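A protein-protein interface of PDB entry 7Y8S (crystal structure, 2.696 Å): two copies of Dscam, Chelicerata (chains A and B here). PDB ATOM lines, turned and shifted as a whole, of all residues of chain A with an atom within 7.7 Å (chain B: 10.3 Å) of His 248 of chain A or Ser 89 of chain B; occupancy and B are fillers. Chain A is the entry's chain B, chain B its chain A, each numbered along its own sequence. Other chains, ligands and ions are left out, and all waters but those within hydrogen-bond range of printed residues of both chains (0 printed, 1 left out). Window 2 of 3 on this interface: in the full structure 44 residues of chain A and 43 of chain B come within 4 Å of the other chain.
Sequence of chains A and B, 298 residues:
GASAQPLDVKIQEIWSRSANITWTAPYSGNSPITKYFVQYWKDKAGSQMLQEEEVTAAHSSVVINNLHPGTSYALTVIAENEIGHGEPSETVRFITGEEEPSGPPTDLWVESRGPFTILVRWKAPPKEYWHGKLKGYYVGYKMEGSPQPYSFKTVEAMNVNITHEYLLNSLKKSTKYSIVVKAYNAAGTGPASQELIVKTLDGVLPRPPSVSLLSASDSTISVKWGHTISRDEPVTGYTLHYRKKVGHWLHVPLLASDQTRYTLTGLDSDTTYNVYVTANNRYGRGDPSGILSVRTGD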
ATOM      1  N   TYR A 242       1.932 -12.167 -13.875  1.00  0.00           N
ATOM      2  CA  TYR A 242       3.223 -12.410 -14.498  1.00  0.00           C
ATOM      3  C   TYR A 242       4.006 -13.436 -13.693  1.00  0.00           C
ATOM      4  O   TYR A 242       3.702 -13.706 -12.530  1.00  0.00           O
ATOM      5  CB  TYR A 242       4.018 -11.109 -14.654  1.00  0.00           C
ATOM      6  CG  TYR A 242       4.507 -10.524 -13.356  1.00  0.00           C
ATOM      7  CD1 TYR A 242       3.636  -9.877 -12.493  1.00  0.00           C
ATOM      8  CD2 TYR A 242       5.843 -10.609 -12.996  1.00  0.00           C
ATOM      9  CE1 TYR A 242       4.081  -9.333 -11.303  1.00  0.00           C
ATOM     10  CE2 TYR A 242       6.297 -10.070 -11.811  1.00  0.00           C
ATOM     11  CZ  TYR A 242       5.411  -9.434 -10.968  1.00  0.00           C
ATOM     12  OH  TYR A 242       5.858  -8.896  -9.785  1.00  0.00           O
ATOM     13  N   ARG A 243       5.021 -14.011 -14.337  1.00  0.00           N
ATOM     14  CA  ARG A 243       5.864 -15.037 -13.732  1.00  0.00           C
ATOM     15  C   ARG A 243       7.088 -15.265 -14.611  1.00  0.00           C
ATOM     16  O   ARG A 243       7.018 -15.131 -15.837  1.00  0.00           O
ATOM     17  CB  ARG A 243       5.103 -16.357 -13.555  1.00  0.00           C
ATOM     18  CG  ARG A 243       4.747 -17.052 -14.873  1.00  0.00           C
ATOM     19  CD  ARG A 243       4.068 -18.394 -14.638  1.00  0.00           C
ATOM     20  NE  ARG A 243       5.001 -19.434 -14.216  1.00  0.00           N
ATOM     21  CZ  ARG A 243       5.779 -20.121 -15.047  1.00  0.00           C
ATOM     22  NH1 ARG A 243       5.742 -19.880 -16.349  1.00  0.00           N
ATOM     23  NH2 ARG A 243       6.599 -21.045 -14.576  1.00  0.00           N
ATOM     24  N   LYS A 244       8.205 -15.610 -13.973  1.00  0.00           N
ATOM     25  CA  LYS A 244       9.337 -16.150 -14.711  1.00  0.00           C
ATOM     26  C   LYS A 244       8.948 -17.486 -15.331  1.00  0.00           C
ATOM     27  O   LYS A 244       8.009 -18.151 -14.888  1.00  0.00           O
ATOM     28  CB  LYS A 244      10.539 -16.358 -13.793  1.00  0.00           C
ATOM     29  CG  LYS A 244      10.983 -15.138 -13.016  1.00  0.00           C
ATOM     30  CD  LYS A 244      12.040 -15.529 -11.993  1.00  0.00           C
ATOM     31  CE  LYS A 244      12.581 -14.312 -11.268  1.00  0.00           C
ATOM     32  NZ  LYS A 244      13.629 -14.667 -10.274  1.00  0.00           N
ATOM     33  N   LYS A 245       9.689 -17.891 -16.363  1.00  0.00           N
ATOM     34  CA  LYS A 245       9.421 -19.195 -16.960  1.00  0.00           C
ATOM     35  C   LYS A 245       9.579 -20.316 -15.940  1.00  0.00           C
ATOM     36  O   LYS A 245       8.930 -21.363 -16.060  1.00  0.00           O
ATOM     37  CB  LYS A 245      10.327 -19.431 -18.165  1.00  0.00           C
ATOM     38  CG  LYS A 245       9.724 -20.403 -19.161  1.00  0.00           C
ATOM     39  CD  LYS A 245      10.373 -20.281 -20.519  1.00  0.00           C
ATOM     40  CE  LYS A 245      11.658 -21.073 -20.580  1.00  0.00           C
ATOM     41  NZ  LYS A 245      11.669 -21.900 -21.810  1.00  0.00           N
ATOM     42  N   VAL A 246      10.427 -20.118 -14.934  1.00  0.00           N
ATOM     43  CA  VAL A 246      10.522 -21.014 -13.786  1.00  0.00           C
ATOM     44  C   VAL A 246      10.249 -20.160 -12.551  1.00  0.00           C
ATOM     45  O   VAL A 246      11.144 -19.495 -12.016  1.00  0.00           O
ATOM     46  CB  VAL A 246      11.876 -21.737 -13.712  1.00  0.00           C
ATOM     47  CG1 VAL A 246      11.960 -22.790 -14.809  1.00  0.00           C
ATOM     48  CG2 VAL A 246      13.042 -20.766 -13.865  1.00  0.00           C
ATOM     49  N   GLY A 247       9.003 -20.152 -12.103  1.00  0.00           N
ATOM     50  CA  GLY A 247       8.626 -19.302 -10.992  1.00  0.00           C
ATOM     51  C   GLY A 247       7.125 -19.256 -10.840  1.00  0.00           C
ATOM     52  O   GLY A 247       6.369 -19.712 -11.704  1.00  0.00           O
ATOM     53  N   HIS A 248       6.702 -18.683  -9.716  1.00  0.00           N
ATOM     54  CA  HIS A 248       5.294 -18.621  -9.356  1.00  0.00           C
ATOM     55  C   HIS A 248       4.627 -17.393  -9.962  1.00  0.00           C
ATOM     56  O   HIS A 248       5.278 -16.386 -10.256  1.00  0.00           O
ATOM     57  CB  HIS A 248       5.118 -18.594  -7.834  1.00  0.00           C
ATOM     58  CG  HIS A 248       5.354 -19.914  -7.172  1.00  0.00           C
ATOM     59  ND1 HIS A 248       6.612 -20.464  -7.037  1.00  0.00           N
ATOM     60  CD2 HIS A 248       4.495 -20.795  -6.605  1.00  0.00           C
ATOM     61  CE1 HIS A 248       6.517 -21.627  -6.417  1.00  0.00           C
ATOM     62  NE2 HIS A 248       5.243 -21.850  -6.144  1.00  0.00           N
ATOM     63  N   TRP A 249       3.312 -17.490 -10.138  1.00  0.00           N
ATOM     64  CA  TRP A 249       2.529 -16.358 -10.607  1.00  0.00           C
ATOM     65  C   TRP A 249       2.465 -15.273  -9.541  1.00  0.00           C
ATOM     66  O   TRP A 249       2.251 -15.549  -8.359  1.00  0.00           O
ATOM     67  CB  TRP A 249       1.115 -16.802 -10.968  1.00  0.00           C
ATOM     68  CG  TRP A 249       0.978 -17.450 -12.309  1.00  0.00           C
ATOM     69  CD1 TRP A 249       0.743 -18.774 -12.561  1.00  0.00           C
ATOM     70  CD2 TRP A 249       1.030 -16.804 -13.589  1.00  0.00           C
ATOM     71  NE1 TRP A 249       0.659 -18.992 -13.918  1.00  0.00           N
ATOM     72  CE2 TRP A 249       0.827 -17.799 -14.570  1.00  0.00           C
ATOM     73  CE3 TRP A 249       1.235 -15.482 -14.002  1.00  0.00           C
ATOM     74  CZ2 TRP A 249       0.832 -17.515 -15.933  1.00  0.00           C
ATOM     75  CZ3 TRP A 249       1.226 -15.203 -15.357  1.00  0.00           C
ATOM     76  CH2 TRP A 249       1.032 -16.215 -16.305  1.00  0.00           C
ATOM     77  N   LEU A 250       2.655 -14.030  -9.964  1.00  0.00           N
ATOM     78  CA  LEU A 250       2.448 -12.871  -9.112  1.00  0.00           C
ATOM     79  C   LEU A 250       1.378 -11.988  -9.741  1.00  0.00           C
ATOM     80  O   LEU A 250       1.180 -12.003 -10.960  1.00  0.00           O
ATOM     81  CB  LEU A 250       3.752 -12.098  -8.904  1.00  0.00           C
ATOM     82  CG  LEU A 250       4.851 -12.934  -8.239  1.00  0.00           C
ATOM     83  CD1 LEU A 250       6.159 -12.871  -9.028  1.00  0.00           C
ATOM     84  CD2 LEU A 250       5.064 -12.497  -6.797  1.00  0.00           C
ATOM     85  N   HIS A 251       0.679 -11.230  -8.897  1.00  0.00           N
ATOM     86  CA  HIS A 251      -0.561 -10.564  -9.281  1.00  0.00           C
ATOM     87  C   HIS A 251      -0.496  -9.097  -8.894  1.00  0.00           C
ATOM     88  O   HIS A 251      -0.373  -8.768  -7.712  1.00  0.00           O
ATOM     89  CB  HIS A 251      -1.765 -11.240  -8.617  1.00  0.00           C
ATOM     90  CG  HIS A 251      -1.895 -12.698  -8.943  1.00  0.00           C
ATOM     91  ND1 HIS A 251      -2.935 -13.203  -9.695  1.00  0.00           N
ATOM     92  CD2 HIS A 251      -1.115 -13.757  -8.623  1.00  0.00           C
ATOM     93  CE1 HIS A 251      -2.790 -14.510  -9.824  1.00  0.00           C
ATOM     94  NE2 HIS A 251      -1.692 -14.872  -9.183  1.00  0.00           N
ATOM     95  N   TYR A 273       9.551 -13.934 -19.188  1.00  0.00           N
ATOM     96  CA  TYR A 273       8.384 -13.759 -18.336  1.00  0.00           C
ATOM     97  C   TYR A 273       7.113 -14.025 -19.132  1.00  0.00           C
ATOM     98  O   TYR A 273       7.033 -13.709 -20.325  1.00  0.00           O
ATOM     99  CB  TYR A 273       8.332 -12.346 -17.748  1.00  0.00           C
ATOM    100  CG  TYR A 273       9.329 -12.091 -16.641  1.00  0.00           C
ATOM    101  CD1 TYR A 273      10.653 -11.778 -16.930  1.00  0.00           C
ATOM    102  CD2 TYR A 273       8.944 -12.149 -15.305  1.00  0.00           C
ATOM    103  CE1 TYR A 273      11.568 -11.537 -15.914  1.00  0.00           C
ATOM    104  CE2 TYR A 273       9.850 -11.910 -14.284  1.00  0.00           C
ATOM    105  CZ  TYR A 273      11.159 -11.605 -14.593  1.00  0.00           C
ATOM    106  OH  TYR A 273      12.060 -11.366 -13.580  1.00  0.00           O
ATOM    107  N   PRO B   6      -2.559 -25.136  -3.992  1.00  0.00           N
ATOM    108  CA  PRO B   6      -2.333 -26.477  -4.539  1.00  0.00           C
ATOM    109  C   PRO B   6      -0.865 -26.872  -4.477  1.00  0.00           C
ATOM    110  O   PRO B   6      -0.072 -26.457  -5.323  1.00  0.00           O
ATOM    111  CB  PRO B   6      -2.809 -26.347  -5.985  1.00  0.00           C
ATOM    112  CG  PRO B   6      -3.851 -25.291  -5.930  1.00  0.00           C
ATOM    113  CD  PRO B   6      -3.379 -24.308  -4.891  1.00  0.00           C
ATOM    114  N   LEU B   7      -0.513 -27.664  -3.472  1.00  0.00           N
ATOM    115  CA  LEU B   7       0.866 -28.086  -3.284  1.00  0.00           C
ATOM    116  C   LEU B   7       1.181 -29.307  -4.144  1.00  0.00           C
ATOM    117  O   LEU B   7       0.307 -30.127  -4.446  1.00  0.00           O
ATOM    118  CB  LEU B   7       1.127 -28.397  -1.808  1.00  0.00           C
ATOM    119  CG  LEU B   7       0.986 -27.227  -0.832  1.00  0.00           C
ATOM    120  CD1 LEU B   7       1.086 -27.699   0.610  1.00  0.00           C
ATOM    121  CD2 LEU B   7       2.039 -26.169  -1.125  1.00  0.00           C
ATOM    122  N   ASP B   8       2.447 -29.407  -4.546  1.00  0.00           N
ATOM    123  CA  ASP B   8       2.995 -30.580  -5.230  1.00  0.00           C
ATOM    124  C   ASP B   8       2.118 -31.012  -6.408  1.00  0.00           C
ATOM    125  O   ASP B   8       1.563 -32.112  -6.438  1.00  0.00           O
ATOM    126  CB  ASP B   8       3.192 -31.731  -4.241  1.00  0.00           C
ATOM    127  CG  ASP B   8       4.238 -31.422  -3.191  1.00  0.00           C
ATOM    128  OD1 ASP B   8       4.935 -30.394  -3.341  1.00  0.00           O
ATOM    129  OD2 ASP B   8       4.355 -32.199  -2.216  1.00  0.00           O
ATOM    130  N   VAL B   9       1.995 -30.112  -7.385  1.00  0.00           N
ATOM    131  CA  VAL B   9       1.284 -30.441  -8.614  1.00  0.00           C
ATOM    132  C   VAL B   9       2.134 -31.396  -9.443  1.00  0.00           C
ATOM    133  O   VAL B   9       3.347 -31.199  -9.598  1.00  0.00           O
ATOM    134  CB  VAL B   9       0.945 -29.164  -9.403  1.00  0.00           C
ATOM    135  CG1 VAL B   9       0.256 -29.512 -10.717  1.00  0.00           C
ATOM    136  CG2 VAL B   9       0.073 -28.238  -8.570  1.00  0.00           C
ATOM    137  N   TRP B  23      -2.556 -33.306  -7.639  1.00  0.00           N
ATOM    138  CA  TRP B  23      -2.117 -32.365  -6.617  1.00  0.00           C
ATOM    139  C   TRP B  23      -2.679 -32.769  -5.259  1.00  0.00           C
ATOM    140  O   TRP B  23      -3.485 -33.697  -5.141  1.00  0.00           O
ATOM    141  CB  TRP B  23      -2.547 -30.934  -6.961  1.00  0.00           C
ATOM    142  CG  TRP B  23      -4.043 -30.751  -7.064  1.00  0.00           C
ATOM    143  CD1 TRP B  23      -4.915 -30.514  -6.043  1.00  0.00           C
ATOM    144  CD2 TRP B  23      -4.833 -30.786  -8.260  1.00  0.00           C
ATOM    145  NE1 TRP B  23      -6.196 -30.396  -6.525  1.00  0.00           N
ATOM    146  CE2 TRP B  23      -6.173 -30.560  -7.885  1.00  0.00           C
ATOM    147  CE3 TRP B  23      -4.537 -30.983  -9.611  1.00  0.00           C
ATOM    148  CZ2 TRP B  23      -7.214 -30.530  -8.810  1.00  0.00           C
ATOM    149  CZ3 TRP B  23      -5.573 -30.952 -10.531  1.00  0.00           C
ATOM    150  CH2 TRP B  23      -6.895 -30.727 -10.127  1.00  0.00           C
ATOM    151  N   THR B  24      -2.227 -32.052  -4.232  1.00  0.00           N
ATOM    152  CA  THR B  24      -2.882 -31.992  -2.934  1.00  0.00           C
ATOM    153  C   THR B  24      -3.090 -30.525  -2.582  1.00  0.00           C
ATOM    154  O   THR B  24      -2.447 -29.638  -3.150  1.00  0.00           O
ATOM    155  CB  THR B  24      -2.064 -32.687  -1.833  1.00  0.00           C
ATOM    156  OG1 THR B  24      -0.744 -32.127  -1.786  1.00  0.00           O
ATOM    157  CG2 THR B  24      -1.976 -34.189  -2.094  1.00  0.00           C
ATOM    158  N   ALA B  25      -4.000 -30.265  -1.640  1.00  0.00           N
ATOM    159  CA  ALA B  25      -4.251 -28.879  -1.265  1.00  0.00           C
ATOM    160  C   ALA B  25      -4.798 -28.766   0.150  1.00  0.00           C
ATOM    161  O   ALA B  25      -5.818 -29.403   0.457  1.00  0.00           O
ATOM    162  CB  ALA B  25      -5.218 -28.215  -2.244  1.00  0.00           C
ATOM    163  N   PRO B  26      -4.154 -27.973   1.024  1.00  0.00           N
ATOM    164  CA  PRO B  26      -4.625 -27.716   2.389  1.00  0.00           C
ATOM    165  C   PRO B  26      -5.754 -26.689   2.437  1.00  0.00           C
ATOM    166  O   PRO B  26      -6.698 -26.875   3.206  1.00  0.00           O
ATOM    167  CB  PRO B  26      -3.374 -27.184   3.092  1.00  0.00           C
ATOM    168  CG  PRO B  26      -2.605 -26.513   2.005  1.00  0.00           C
ATOM    169  CD  PRO B  26      -2.856 -27.320   0.757  1.00  0.00           C
ATOM    170  N   ILE B  33     -11.760 -24.513   0.370  1.00  0.00           N
ATOM    171  CA  ILE B  33     -11.442 -23.982  -0.950  1.00  0.00           C
ATOM    172  C   ILE B  33     -12.666 -24.055  -1.866  1.00  0.00           C
ATOM    173  O   ILE B  33     -13.430 -25.020  -1.824  1.00  0.00           O
ATOM    174  CB  ILE B  33     -10.213 -24.709  -1.552  1.00  0.00           C
ATOM    175  CG1 ILE B  33     -10.230 -26.203  -1.211  1.00  0.00           C
ATOM    176  CG2 ILE B  33      -8.922 -24.094  -1.049  1.00  0.00           C
ATOM    177  CD1 ILE B  33     -11.392 -26.955  -1.774  1.00  0.00           C
ATOM    178  N   LYS B  35     -13.107 -23.885  -5.517  1.00  0.00           N
ATOM    179  CA  LYS B  35     -12.991 -24.764  -6.664  1.00  0.00           C
ATOM    180  C   LYS B  35     -11.506 -24.862  -6.966  1.00  0.00           C
ATOM    181  O   LYS B  35     -10.683 -24.210  -6.317  1.00  0.00           O
ATOM    182  CB  LYS B  35     -13.767 -24.207  -7.858  1.00  0.00           C
ATOM    183  CG  LYS B  35     -13.325 -22.793  -8.211  1.00  0.00           C
ATOM    184  CD  LYS B  35     -14.449 -21.976  -8.794  1.00  0.00           C
ATOM    185  CE  LYS B  35     -14.674 -22.359 -10.242  1.00  0.00           C
ATOM    186  NZ  LYS B  35     -15.149 -21.230 -11.096  1.00  0.00           N
ATOM    187  N   TYR B  36     -11.154 -25.676  -7.952  1.00  0.00           N
ATOM    188  CA  TYR B  36      -9.804 -25.647  -8.488  1.00  0.00           C
ATOM    189  C   TYR B  36      -9.855 -25.180  -9.935  1.00  0.00           C
ATOM    190  O   TYR B  36     -10.741 -25.578 -10.700  1.00  0.00           O
ATOM    191  CB  TYR B  36      -9.120 -27.006  -8.387  1.00  0.00           C
ATOM    192  CG  TYR B  36      -8.857 -27.489  -6.981  1.00  0.00           C
ATOM    193  CD1 TYR B  36      -7.851 -26.930  -6.197  1.00  0.00           C
ATOM    194  CD2 TYR B  36      -9.604 -28.526  -6.444  1.00  0.00           C
ATOM    195  CE1 TYR B  36      -7.606 -27.392  -4.907  1.00  0.00           C
ATOM    196  CE2 TYR B  36      -9.371 -28.992  -5.162  1.00  0.00           C
ATOM    197  CZ  TYR B  36      -8.374 -28.425  -4.396  1.00  0.00           C
ATOM    198  OH  TYR B  36      -8.155 -28.896  -3.121  1.00  0.00           O
ATOM    199  N   PHE B  37      -8.902 -24.324 -10.287  1.00  0.00           N
ATOM    200  CA  PHE B  37      -8.845 -23.654 -11.577  1.00  0.00           C
ATOM    201  C   PHE B  37      -7.570 -24.098 -12.280  1.00  0.00           C
ATOM    202  O   PHE B  37      -6.474 -23.966 -11.722  1.00  0.00           O
ATOM    203  CB  PHE B  37      -8.870 -22.138 -11.374  1.00  0.00           C
ATOM    204  CG  PHE B  37      -9.362 -21.365 -12.555  1.00  0.00           C
ATOM    205  CD1 PHE B  37     -10.503 -21.754 -13.237  1.00  0.00           C
ATOM    206  CD2 PHE B  37      -8.693 -20.226 -12.969  1.00  0.00           C
ATOM    207  CE1 PHE B  37     -10.958 -21.029 -14.322  1.00  0.00           C
ATOM    208  CE2 PHE B  37      -9.141 -19.497 -14.051  1.00  0.00           C
ATOM    209  CZ  PHE B  37     -10.275 -19.898 -14.728  1.00  0.00           C
ATOM    210  N   VAL B  38      -7.709 -24.633 -13.492  1.00  0.00           N
ATOM    211  CA  VAL B  38      -6.603 -25.259 -14.213  1.00  0.00           C
ATOM    212  C   VAL B  38      -6.341 -24.470 -15.489  1.00  0.00           C
ATOM    213  O   VAL B  38      -7.118 -24.553 -16.451  1.00  0.00           O
ATOM    214  CB  VAL B  38      -6.889 -26.732 -14.527  1.00  0.00           C
ATOM    215  CG1 VAL B  38      -5.765 -27.323 -15.358  1.00  0.00           C
ATOM    216  CG2 VAL B  38      -7.066 -27.516 -13.237  1.00  0.00           C
ATOM    217  N   GLN B  39      -5.248 -23.710 -15.505  1.00  0.00           N
ATOM    218  CA  GLN B  39      -4.814 -22.975 -16.686  1.00  0.00           C
ATOM    219  C   GLN B  39      -3.693 -23.737 -17.378  1.00  0.00           C
ATOM    220  O   GLN B  39      -2.822 -24.310 -16.718  1.00  0.00           O
ATOM    221  CB  GLN B  39      -4.322 -21.570 -16.324  1.00  0.00           C
ATOM    222  CG  GLN B  39      -5.297 -20.738 -15.514  1.00  0.00           C
ATOM    223  CD  GLN B  39      -4.702 -19.412 -15.089  1.00  0.00           C
ATOM    224  OE1 GLN B  39      -3.712 -19.368 -14.360  1.00  0.00           O
ATOM    225  NE2 GLN B  39      -5.300 -18.320 -15.546  1.00  0.00           N
ATOM    226  N   TRP B  41      -1.289 -23.650 -21.347  1.00  0.00           N
ATOM    227  CA  TRP B  41      -0.996 -22.994 -22.613  1.00  0.00           C
ATOM    228  C   TRP B  41       0.237 -23.624 -23.249  1.00  0.00           C
ATOM    229  O   TRP B  41       1.041 -24.282 -22.582  1.00  0.00           O
ATOM    230  CB  TRP B  41      -0.789 -21.488 -22.425  1.00  0.00           C
ATOM    231  CG  TRP B  41       0.365 -21.116 -21.539  1.00  0.00           C
ATOM    232  CD1 TRP B  41       1.571 -20.623 -21.935  1.00  0.00           C
ATOM    233  CD2 TRP B  41       0.414 -21.183 -20.104  1.00  0.00           C
ATOM    234  NE1 TRP B  41       2.370 -20.384 -20.840  1.00  0.00           N
ATOM    235  CE2 TRP B  41       1.684 -20.720 -19.705  1.00  0.00           C
ATOM    236  CE3 TRP B  41      -0.494 -21.590 -19.119  1.00  0.00           C
ATOM    237  CZ2 TRP B  41       2.072 -20.651 -18.366  1.00  0.00           C
ATOM    238  CZ3 TRP B  41      -0.106 -21.525 -17.788  1.00  0.00           C
ATOM    239  CH2 TRP B  41       1.166 -21.061 -17.427  1.00  0.00           C
ATOM    240  N   LEU B  75       1.407 -25.323 -17.320  1.00  0.00           N
ATOM    241  CA  LEU B  75       0.126 -25.578 -16.678  1.00  0.00           C
ATOM    242  C   LEU B  75       0.143 -25.060 -15.248  1.00  0.00           C
ATOM    243  O   LEU B  75       1.158 -25.167 -14.553  1.00  0.00           O
ATOM    244  CB  LEU B  75      -0.201 -27.075 -16.699  1.00  0.00           C
ATOM    245  CG  LEU B  75      -1.572 -27.532 -16.199  1.00  0.00           C
ATOM    246  CD1 LEU B  75      -2.033 -28.729 -17.011  1.00  0.00           C
ATOM    247  CD2 LEU B  75      -1.538 -27.883 -14.722  1.00  0.00           C
ATOM    248  N   THR B  76      -0.994 -24.511 -14.815  1.00  0.00           N
ATOM    249  CA  THR B  76      -1.153 -23.960 -13.477  1.00  0.00           C
ATOM    250  C   THR B  76      -2.464 -24.449 -12.880  1.00  0.00           C
ATOM    251  O   THR B  76      -3.476 -24.544 -13.580  1.00  0.00           O
ATOM    252  CB  THR B  76      -1.147 -22.421 -13.488  1.00  0.00           C
ATOM    253  OG1 THR B  76       0.021 -21.945 -14.166  1.00  0.00           O
ATOM    254  CG2 THR B  76      -1.141 -21.882 -12.068  1.00  0.00           C
ATOM    255  N   VAL B  77      -2.439 -24.763 -11.587  1.00  0.00           N
ATOM    256  CA  VAL B  77      -3.637 -25.114 -10.834  1.00  0.00           C
ATOM    257  C   VAL B  77      -3.800 -24.099  -9.709  1.00  0.00           C
ATOM    258  O   VAL B  77      -2.848 -23.828  -8.968  1.00  0.00           O
ATOM    259  CB  VAL B  77      -3.564 -26.547 -10.277  1.00  0.00           C
ATOM    260  CG1 VAL B  77      -4.864 -26.909  -9.584  1.00  0.00           C
ATOM    261  CG2 VAL B  77      -3.276 -27.531 -11.396  1.00  0.00           C
ATOM    262  N   ILE B  78      -5.001 -23.533  -9.591  1.00  0.00           N
ATOM    263  CA  ILE B  78      -5.301 -22.515  -8.592  1.00  0.00           C
ATOM    264  C   ILE B  78      -6.459 -22.997  -7.728  1.00  0.00           C
ATOM    265  O   ILE B  78      -7.471 -23.484  -8.251  1.00  0.00           O
ATOM    266  CB  ILE B  78      -5.642 -21.156  -9.234  1.00  0.00           C
ATOM    267  CG1 ILE B  78      -4.684 -20.841 -10.385  1.00  0.00           C
ATOM    268  CG2 ILE B  78      -5.607 -20.054  -8.181  1.00  0.00           C
ATOM    269  CD1 ILE B  78      -4.698 -19.388 -10.820  1.00  0.00           C
ATOM    270  N   ALA B  79      -6.314 -22.847  -6.414  1.00  0.00           N
ATOM    271  CA  ALA B  79      -7.394 -23.147  -5.480  1.00  0.00           C
ATOM    272  C   ALA B  79      -8.151 -21.873  -5.112  1.00  0.00           C
ATOM    273  O   ALA B  79      -7.644 -21.033  -4.366  1.00  0.00           O
ATOM    274  CB  ALA B  79      -6.849 -23.819  -4.229  1.00  0.00           C
ATOM    275  N   SER B  89      -0.649 -20.116  -8.607  1.00  0.00           N
ATOM    276  CA  SER B  89      -0.485 -20.843  -7.351  1.00  0.00           C
ATOM    277  C   SER B  89       0.671 -21.842  -7.431  1.00  0.00           C
ATOM    278  O   SER B  89       1.496 -21.915  -6.519  1.00  0.00           O
ATOM    279  CB  SER B  89      -1.779 -21.563  -6.979  1.00  0.00           C
ATOM    280  OG  SER B  89      -1.916 -21.653  -5.572  1.00  0.00           O
ATOM    281  N   GLU B  90       0.718 -22.612  -8.520  1.00  0.00           N
ATOM    282  CA  GLU B  90       1.833 -23.517  -8.785  1.00  0.00           C
ATOM    283  C   GLU B  90       1.801 -23.924 -10.253  1.00  0.00           C
ATOM    284  O   GLU B  90       0.746 -24.319 -10.763  1.00  0.00           O
ATOM    285  CB  GLU B  90       1.780 -24.754  -7.886  1.00  0.00           C
ATOM    286  CG  GLU B  90       3.088 -25.525  -7.839  1.00  0.00           C
ATOM    287  CD  GLU B  90       3.134 -26.546  -6.716  1.00  0.00           C
ATOM    288  OE1 GLU B  90       2.967 -26.153  -5.538  1.00  0.00           O
ATOM    289  OE2 GLU B  90       3.335 -27.745  -7.016  1.00  0.00           O
ATOM    290  N   THR B  91       2.953 -23.829 -10.922  1.00  0.00           N
ATOM    291  CA  THR B  91       3.049 -23.994 -12.368  1.00  0.00           C
ATOM    292  C   THR B  91       4.075 -25.063 -12.716  1.00  0.00           C
ATOM    293  O   THR B  91       5.205 -25.030 -12.217  1.00  0.00           O
ATOM    294  CB  THR B  91       3.435 -22.679 -13.051  1.00  0.00           C
ATOM    295  OG1 THR B  91       2.436 -21.687 -12.786  1.00  0.00           O
ATOM    296  CG2 THR B  91       3.570 -22.882 -14.557  1.00  0.00           C
ATOM    297  N   VAL B  92       3.686 -25.989 -13.597  1.00  0.00           N
ATOM    298  CA  VAL B  92       4.540 -27.080 -14.050  1.00  0.00           C
ATOM    299  C   VAL B  92       4.593 -27.060 -15.571  1.00  0.00           C
ATOM    300  O   VAL B  92       3.787 -26.408 -16.235  1.00  0.00           O
ATOM    301  CB  VAL B  92       4.046 -28.453 -13.553  1.00  0.00           C
ATOM    302  CG1 VAL B  92       3.900 -28.448 -12.035  1.00  0.00           C
ATOM    303  CG2 VAL B  92       2.737 -28.803 -14.222  1.00  0.00           C
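OG1 of Thr 91 of chain B lies close to NE1 of Trp 249 of chain A, 3.4 Å away.
OG1 of Thr 76 of chain B lies within hydrogen-bond range of NE1 of Trp 249 of chain A (3.0 Å).
OG1 of Thr 91 of chain B is in hydrogen-bond range of OG1 of Thr 76 of chain B.
The guanidinium group of Arg 243 of chain A sits at hydrogen-bond distance from the backbone carbonyl oxygen of Gly 247 of chain A, 2.9 Å away.
The guanidinium group of Arg 243 of chain A sits at hydrogen-bond distance from the backbone carbonyl oxygen of Lys 245 of chain A, at 2.8 Å.
O of Gln 39 of chain B sits at hydrogen-bond distance from N of Thr 76 of chain B (2.6 Å).
Among the printed residues, pairs that only touch across the chains: Arg 243 of chain A with Thr 91 of chain B (3.5 Å), His 248 of chain A with Ser 89 of chain B (3.2 Å) and Trp 249 of chain A with Trp 41 of chain B (3.9 Å).
Of chain B, only Ser 89 comes within 4 Å of His 248 of chain A.
Ser 89 of chain B touches just one residue of chain A: His 248.
Leu 250 of chain A touches none of the printed residues of chain B.
Of the printed residues of chain A, Thr 76 of chain B touches Trp 249.
Printed residues of chain A within 4 Å of Thr 91 of chain B: Arg 243 (3.5 Å) and Trp 249 (3.4 Å).
Hydrophobic or aromatic side chains of chain A that line the printed part of chain B: His 248 and Trp 249.
Along chain A the printed residues that touch a printed residue of chain B span positions 243 to 249.
Among the printed residues, no Asp or Glu carboxylate lies within 4 Å of a Lys or Arg side-chain nitrogen of the other chain.
No position is printed for both chains.
Of the 5 pairs that touch across the chains among the printed residues, none has its exchanged pair printed and touching as well.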
